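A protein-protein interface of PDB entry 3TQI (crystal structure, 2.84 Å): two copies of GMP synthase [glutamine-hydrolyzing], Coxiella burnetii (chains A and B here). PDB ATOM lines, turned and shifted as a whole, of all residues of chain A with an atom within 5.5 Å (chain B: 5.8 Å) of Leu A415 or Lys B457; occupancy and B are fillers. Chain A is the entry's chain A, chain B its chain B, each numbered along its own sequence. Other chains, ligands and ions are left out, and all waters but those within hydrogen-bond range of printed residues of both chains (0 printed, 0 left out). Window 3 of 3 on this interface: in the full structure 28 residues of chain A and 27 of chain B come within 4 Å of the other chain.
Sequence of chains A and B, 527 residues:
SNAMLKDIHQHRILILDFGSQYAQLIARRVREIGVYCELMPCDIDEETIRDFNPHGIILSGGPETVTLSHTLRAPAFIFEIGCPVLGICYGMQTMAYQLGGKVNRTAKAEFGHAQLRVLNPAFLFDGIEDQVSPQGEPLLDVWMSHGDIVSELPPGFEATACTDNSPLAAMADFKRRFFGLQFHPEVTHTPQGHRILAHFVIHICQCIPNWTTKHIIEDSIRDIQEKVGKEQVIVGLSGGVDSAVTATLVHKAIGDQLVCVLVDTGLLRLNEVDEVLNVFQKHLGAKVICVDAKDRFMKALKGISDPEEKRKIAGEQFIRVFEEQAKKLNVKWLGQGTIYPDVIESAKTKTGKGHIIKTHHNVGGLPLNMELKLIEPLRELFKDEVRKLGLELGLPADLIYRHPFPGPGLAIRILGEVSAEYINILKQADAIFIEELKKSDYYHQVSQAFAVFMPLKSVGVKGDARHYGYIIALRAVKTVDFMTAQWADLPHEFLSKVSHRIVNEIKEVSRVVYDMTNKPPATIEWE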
ATOM      1  N   SER A 305       1.667 -19.561   4.504  1.00  0.00           N
ATOM      2  CA  SER A 305       2.402 -18.966   5.611  1.00  0.00           C
ATOM      3  C   SER A 305       1.577 -17.867   6.273  1.00  0.00           C
ATOM      4  O   SER A 305       1.643 -17.695   7.487  1.00  0.00           O
ATOM      5  CB  SER A 305       3.729 -18.405   5.116  1.00  0.00           C
ATOM      6  OG  SER A 305       4.505 -19.423   4.511  1.00  0.00           O
ATOM      7  N   LYS A 310      -4.292 -19.260   7.187  1.00  0.00           N
ATOM      8  CA  LYS A 310      -4.244 -20.512   7.942  1.00  0.00           C
ATOM      9  C   LYS A 310      -5.551 -20.672   8.686  1.00  0.00           C
ATOM     10  O   LYS A 310      -6.187 -21.725   8.618  1.00  0.00           O
ATOM     11  CB  LYS A 310      -3.069 -20.537   8.932  1.00  0.00           C
ATOM     12  CG  LYS A 310      -1.702 -20.719   8.272  1.00  0.00           C
ATOM     13  CD  LYS A 310      -0.616 -21.167   9.250  1.00  0.00           C
ATOM     14  CE  LYS A 310      -0.042 -20.019  10.058  1.00  0.00           C
ATOM     15  NZ  LYS A 310       1.053 -20.457  10.957  1.00  0.00           N
ATOM     16  N   ARG A 413       0.706 -20.947  16.619  1.00  0.00           N
ATOM     17  CA  ARG A 413       1.746 -21.606  17.434  1.00  0.00           C
ATOM     18  C   ARG A 413       2.863 -22.252  16.619  1.00  0.00           C
ATOM     19  O   ARG A 413       3.861 -22.695  17.175  1.00  0.00           O
ATOM     20  CB  ARG A 413       1.133 -22.638  18.374  1.00  0.00           C
ATOM     21  CG  ARG A 413      -0.125 -22.136  19.026  1.00  0.00           C
ATOM     22  CD  ARG A 413      -0.391 -22.792  20.342  1.00  0.00           C
ATOM     23  NE  ARG A 413      -1.398 -22.051  21.084  1.00  0.00           N
ATOM     24  CZ  ARG A 413      -1.920 -22.458  22.231  1.00  0.00           C
ATOM     25  NH1 ARG A 413      -1.529 -23.606  22.778  1.00  0.00           N
ATOM     26  NH2 ARG A 413      -2.840 -21.718  22.835  1.00  0.00           N
ATOM     27  N   ILE A 414       2.650 -22.347  15.311  1.00  0.00           N
ATOM     28  CA  ILE A 414       3.700 -22.540  14.342  1.00  0.00           C
ATOM     29  C   ILE A 414       3.683 -21.272  13.501  1.00  0.00           C
ATOM     30  O   ILE A 414       2.649 -20.924  12.933  1.00  0.00           O
ATOM     31  CB  ILE A 414       3.430 -23.762  13.461  1.00  0.00           C
ATOM     32  CG1 ILE A 414       3.247 -25.004  14.331  1.00  0.00           C
ATOM     33  CG2 ILE A 414       4.568 -23.978  12.481  1.00  0.00           C
ATOM     34  CD1 ILE A 414       3.017 -26.277  13.549  1.00  0.00           C
ATOM     35  N   LEU A 415       4.814 -20.566  13.455  1.00  0.00           N
ATOM     36  CA  LEU A 415       4.889 -19.270  12.776  1.00  0.00           C
ATOM     37  C   LEU A 415       4.863 -19.411  11.262  1.00  0.00           C
ATOM     38  O   LEU A 415       4.099 -18.724  10.587  1.00  0.00           O
ATOM     39  CB  LEU A 415       6.140 -18.499  13.200  1.00  0.00           C
ATOM     40  CG  LEU A 415       6.043 -17.823  14.564  1.00  0.00           C
ATOM     41  CD1 LEU A 415       7.403 -17.297  14.987  1.00  0.00           C
ATOM     42  CD2 LEU A 415       5.010 -16.703  14.541  1.00  0.00           C
ATOM     43  N   GLY A 416       5.691 -20.298  10.728  1.00  0.00           N
ATOM     44  CA  GLY A 416       5.770 -20.473   9.284  1.00  0.00           C
ATOM     45  C   GLY A 416       4.639 -21.322   8.732  1.00  0.00           C
ATOM     46  O   GLY A 416       3.514 -21.304   9.232  1.00  0.00           O
ATOM     47  N   GLU A 417       4.952 -22.059   7.675  1.00  0.00           N
ATOM     48  CA  GLU A 417       4.069 -23.090   7.155  1.00  0.00           C
ATOM     49  C   GLU A 417       3.924 -24.164   8.225  1.00  0.00           C
ATOM     50  O   GLU A 417       4.891 -24.482   8.912  1.00  0.00           O
ATOM     51  CB  GLU A 417       4.647 -23.662   5.839  1.00  0.00           C
ATOM     52  CG  GLU A 417       4.903 -25.185   5.803  1.00  0.00           C
ATOM     53  CD  GLU A 417       5.811 -25.620   4.653  1.00  0.00           C
ATOM     54  OE1 GLU A 417       5.325 -26.305   3.726  1.00  0.00           O
ATOM     55  OE2 GLU A 417       7.017 -25.285   4.688  1.00  0.00           O
ATOM     56  N   PHE A 453       6.481 -22.610  18.042  1.00  0.00           N
ATOM     57  CA  PHE A 453       7.586 -23.146  17.255  1.00  0.00           C
ATOM     58  C   PHE A 453       7.973 -22.154  16.168  1.00  0.00           C
ATOM     59  O   PHE A 453       7.177 -21.846  15.279  1.00  0.00           O
ATOM     60  CB  PHE A 453       7.153 -24.468  16.618  1.00  0.00           C
ATOM     61  CG  PHE A 453       8.180 -25.085  15.711  1.00  0.00           C
ATOM     62  CD1 PHE A 453       9.045 -26.059  16.185  1.00  0.00           C
ATOM     63  CD2 PHE A 453       8.255 -24.719  14.378  1.00  0.00           C
ATOM     64  CE1 PHE A 453       9.981 -26.649  15.353  1.00  0.00           C
ATOM     65  CE2 PHE A 453       9.190 -25.298  13.536  1.00  0.00           C
ATOM     66  CZ  PHE A 453      10.057 -26.267  14.024  1.00  0.00           C
ATOM     67  N   MET A 454       9.203 -21.658  16.257  1.00  0.00           N
ATOM     68  CA  MET A 454       9.774 -20.776  15.246  1.00  0.00           C
ATOM     69  C   MET A 454      10.697 -21.622  14.375  1.00  0.00           C
ATOM     70  O   MET A 454      11.579 -22.306  14.896  1.00  0.00           O
ATOM     71  CB  MET A 454      10.579 -19.653  15.900  1.00  0.00           C
ATOM     72  CG  MET A 454      10.018 -19.128  17.218  1.00  0.00           C
ATOM     73  SD  MET A 454      10.746 -17.548  17.658  1.00  0.00           S
ATOM     74  CE  MET A 454      10.928 -17.756  19.408  1.00  0.00           C
ATOM     75  N   PRO A 455      10.501 -21.597  13.049  1.00  0.00           N
ATOM     76  CA  PRO A 455      11.341 -22.406  12.179  1.00  0.00           C
ATOM     77  C   PRO A 455      12.629 -21.691  11.794  1.00  0.00           C
ATOM     78  O   PRO A 455      12.938 -21.595  10.606  1.00  0.00           O
ATOM     79  CB  PRO A 455      10.452 -22.597  10.951  1.00  0.00           C
ATOM     80  CG  PRO A 455       9.703 -21.316  10.867  1.00  0.00           C
ATOM     81  CD  PRO A 455       9.431 -20.921  12.293  1.00  0.00           C
ATOM     82  N   TRP A 526       0.337 -15.726  19.135  1.00  0.00           N
ATOM     83  CA  TRP A 526       1.120 -15.160  18.045  1.00  0.00           C
ATOM     84  C   TRP A 526       0.329 -15.399  16.762  1.00  0.00           C
ATOM     85  O   TRP A 526       0.615 -14.818  15.729  1.00  0.00           O
ATOM     86  CB  TRP A 526       2.499 -15.829  17.963  1.00  0.00           C
ATOM     87  CG  TRP A 526       3.358 -15.722  19.225  1.00  0.00           C
ATOM     88  CD1 TRP A 526       2.923 -15.534  20.501  1.00  0.00           C
ATOM     89  CD2 TRP A 526       4.788 -15.829  19.310  1.00  0.00           C
ATOM     90  NE1 TRP A 526       3.982 -15.500  21.367  1.00  0.00           N
ATOM     91  CE2 TRP A 526       5.139 -15.682  20.664  1.00  0.00           C
ATOM     92  CE3 TRP A 526       5.806 -16.035  18.370  1.00  0.00           C
ATOM     93  CZ2 TRP A 526       6.461 -15.732  21.108  1.00  0.00           C
ATOM     94  CZ3 TRP A 526       7.128 -16.088  18.815  1.00  0.00           C
ATOM     95  CH2 TRP A 526       7.438 -15.936  20.174  1.00  0.00           C
ATOM     96  N   MET B 454      15.185 -11.714  14.912  1.00  0.00           N
ATOM     97  CA  MET B 454      14.584 -12.841  14.201  1.00  0.00           C
ATOM     98  C   MET B 454      13.667 -12.297  13.123  1.00  0.00           C
ATOM     99  O   MET B 454      12.744 -11.539  13.430  1.00  0.00           O
ATOM    100  CB  MET B 454      13.784 -13.703  15.158  1.00  0.00           C
ATOM    101  CG  MET B 454      14.479 -13.938  16.469  1.00  0.00           C
ATOM    102  SD  MET B 454      13.679 -15.225  17.390  1.00  0.00           S
ATOM    103  CE  MET B 454      14.179 -14.765  19.023  1.00  0.00           C
ATOM    104  N   PRO B 455      13.900 -12.688  11.857  1.00  0.00           N
ATOM    105  CA  PRO B 455      13.145 -12.128  10.750  1.00  0.00           C
ATOM    106  C   PRO B 455      11.792 -12.795  10.519  1.00  0.00           C
ATOM    107  O   PRO B 455      11.427 -13.017   9.369  1.00  0.00           O
ATOM    108  CB  PRO B 455      14.069 -12.399   9.560  1.00  0.00           C
ATOM    109  CG  PRO B 455      14.695 -13.684   9.893  1.00  0.00           C
ATOM    110  CD  PRO B 455      14.932 -13.626  11.375  1.00  0.00           C
ATOM    111  N   LEU B 456      11.033 -13.086  11.572  1.00  0.00           N
ATOM    112  CA  LEU B 456       9.847 -13.920  11.397  1.00  0.00           C
ATOM    113  C   LEU B 456       8.502 -13.205  11.415  1.00  0.00           C
ATOM    114  O   LEU B 456       7.660 -13.473  10.553  1.00  0.00           O
ATOM    115  CB  LEU B 456       9.852 -15.099  12.373  1.00  0.00           C
ATOM    116  CG  LEU B 456      10.474 -16.356  11.753  1.00  0.00           C
ATOM    117  CD1 LEU B 456      10.536 -17.465  12.782  1.00  0.00           C
ATOM    118  CD2 LEU B 456       9.706 -16.819  10.518  1.00  0.00           C
ATOM    119  N   LYS B 457       8.299 -12.316  12.381  1.00  0.00           N
ATOM    120  CA  LYS B 457       7.049 -11.533  12.500  1.00  0.00           C
ATOM    121  C   LYS B 457       5.894 -12.249  13.219  1.00  0.00           C
ATOM    122  O   LYS B 457       5.658 -13.442  13.030  1.00  0.00           O
ATOM    123  CB  LYS B 457       6.552 -10.975  11.145  1.00  0.00           C
ATOM    124  CG  LYS B 457       7.548 -10.046  10.440  1.00  0.00           C
ATOM    125  CD  LYS B 457       6.903  -9.123   9.404  1.00  0.00           C
ATOM    126  CE  LYS B 457       6.625  -9.837   8.090  1.00  0.00           C
ATOM    127  NZ  LYS B 457       5.817  -9.003   7.140  1.00  0.00           N
ATOM    128  N   SER B 458       5.178 -11.481  14.037  1.00  0.00           N
ATOM    129  CA  SER B 458       4.036 -11.972  14.795  1.00  0.00           C
ATOM    130  C   SER B 458       3.041 -10.842  15.010  1.00  0.00           C
ATOM    131  O   SER B 458       3.327  -9.701  14.690  1.00  0.00           O
ATOM    132  CB  SER B 458       4.491 -12.501  16.148  1.00  0.00           C
ATOM    133  OG  SER B 458       4.589 -11.451  17.091  1.00  0.00           O
ATOM    134  N   VAL B 459       1.886 -11.164  15.582  1.00  0.00           N
ATOM    135  CA  VAL B 459       0.821 -10.183  15.787  1.00  0.00           C
ATOM    136  C   VAL B 459       1.058  -9.388  17.070  1.00  0.00           C
ATOM    137  O   VAL B 459       0.723  -8.208  17.147  1.00  0.00           O
ATOM    138  CB  VAL B 459      -0.565 -10.868  15.844  1.00  0.00           C
ATOM    139  CG1 VAL B 459      -1.668  -9.840  16.039  1.00  0.00           C
ATOM    140  CG2 VAL B 459      -0.817 -11.671  14.582  1.00  0.00           C
ATOM    141  N   TYR B 468       1.473  -6.857  12.135  1.00  0.00           N
ATOM    142  CA  TYR B 468       2.557  -7.829  12.308  1.00  0.00           C
ATOM    143  C   TYR B 468       3.943  -7.205  12.169  1.00  0.00           C
ATOM    144  O   TYR B 468       4.195  -6.441  11.244  1.00  0.00           O
ATOM    145  CB  TYR B 468       2.436  -9.031  11.345  1.00  0.00           C
ATOM    146  CG  TYR B 468       1.367  -8.913  10.280  1.00  0.00           C
ATOM    147  CD1 TYR B 468       1.495  -8.005   9.222  1.00  0.00           C
ATOM    148  CD2 TYR B 468       0.216  -9.722  10.324  1.00  0.00           C
ATOM    149  CE1 TYR B 468       0.491  -7.895   8.233  1.00  0.00           C
ATOM    150  CE2 TYR B 468      -0.784  -9.622   9.348  1.00  0.00           C
ATOM    151  CZ  TYR B 468      -0.640  -8.709   8.307  1.00  0.00           C
ATOM    152  OH  TYR B 468      -1.625  -8.616   7.348  1.00  0.00           O
ATOM    153  N   GLY B 469       4.841  -7.556  13.086  1.00  0.00           N
ATOM    154  CA  GLY B 469       6.218  -7.058  13.062  1.00  0.00           C
ATOM    155  C   GLY B 469       7.228  -8.076  13.564  1.00  0.00           C
ATOM    156  O   GLY B 469       6.851  -9.096  14.130  1.00  0.00           O
ATOM    157  N   TYR B 470       8.513  -7.770  13.390  1.00  0.00           N
ATOM    158  CA  TYR B 470       9.598  -8.717  13.678  1.00  0.00           C
ATOM    159  C   TYR B 470       9.798  -8.981  15.172  1.00  0.00           C
ATOM    160  O   TYR B 470       9.374  -8.202  16.011  1.00  0.00           O
ATOM    161  CB  TYR B 470      10.917  -8.209  13.085  1.00  0.00           C
ATOM    162  CG  TYR B 470      10.923  -8.047  11.577  1.00  0.00           C
ATOM    163  CD1 TYR B 470      10.777  -9.147  10.737  1.00  0.00           C
ATOM    164  CD2 TYR B 470      11.105  -6.795  10.994  1.00  0.00           C
ATOM    165  CE1 TYR B 470      10.796  -9.001   9.353  1.00  0.00           C
ATOM    166  CE2 TYR B 470      11.123  -6.638   9.615  1.00  0.00           C
ATOM    167  CZ  TYR B 470      10.970  -7.742   8.798  1.00  0.00           C
ATOM    168  OH  TYR B 470      10.993  -7.582   7.428  1.00  0.00           O
ATOM    169  N   ILE B 471      10.474 -10.077  15.499  1.00  0.00           N
ATOM    170  CA  ILE B 471      10.660 -10.477  16.894  1.00  0.00           C
ATOM    171  C   ILE B 471      12.114 -10.287  17.312  1.00  0.00           C
ATOM    172  O   ILE B 471      13.029 -10.583  16.538  1.00  0.00           O
ATOM    173  CB  ILE B 471      10.264 -11.955  17.115  1.00  0.00           C
ATOM    174  CG1 ILE B 471       8.962 -12.277  16.375  1.00  0.00           C
ATOM    175  CG2 ILE B 471      10.135 -12.258  18.604  1.00  0.00           C
ATOM    176  CD1 ILE B 471       8.497 -13.707  16.550  1.00  0.00           C
ATOM    177  N   SER B 510       6.930  -5.239  17.476  1.00  0.00           N
ATOM    178  CA  SER B 510       5.873  -6.079  18.073  1.00  0.00           C
ATOM    179  C   SER B 510       6.440  -7.339  18.720  1.00  0.00           C
ATOM    180  O   SER B 510       6.901  -8.235  18.023  1.00  0.00           O
ATOM    181  CB  SER B 510       4.841  -6.513  17.016  1.00  0.00           C
ATOM    182  OG  SER B 510       5.242  -7.708  16.344  1.00  0.00           O
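SD of Met B454 lies close to SD of Met A454 (3.8 Å).
The backbone NH (N) of Leu A415 lies within hydrogen-bond range of the backbone carbonyl oxygen (O) of Phe A453 (3.2 Å).
The backbone NH of Met B454 is in hydrogen-bond range of the backbone carbonyl oxygen of Ile B471 (2.9 Å).
CD1 of Leu A415 touches CD1 of Leu B456, 3.8 Å away.
Lys B457 touches Leu A415 (O to CD2, 3.7 Å).
Met A454 touches Leu B456.
Pro A455 touches Leu B456 (CD to CD1, 3.7 Å).
Val B459 touches Trp A526 (CG2 to O, 3.6 Å).
Trp A526 touches Ile B471 (CZ3 to CD1, 3.6 Å).
Lys A310 touches none of the printed residues of chain B.
Of chain B, only Leu B456 (3.8 Å) and Lys B457 (3.7 Å) come within 4 Å of Leu A415.
Of the printed residues of chain B, Pro A455 touches Leu B456.
Printed residues of chain A within 4 Å of Leu B456: Leu A415 (3.8 Å), Met A454 (3.8 Å) and Pro A455 (3.7 Å).
Lys B457 touches one residue of chain A.
The nearest residue of chain B that does not touch Leu A415 is Ile B471 (4.1 Å).
Of the 11 printed residues of chain B, 5 touch a printed residue of chain A.
Along chain B the printed residues that touch a printed residue of chain A span positions 454 to 471.
Met B454 touches its own counterpart, Met A454.
Of the 7 pairs that touch across the chains among the printed residues, 1 has its exchanged pair printed and touching as well.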
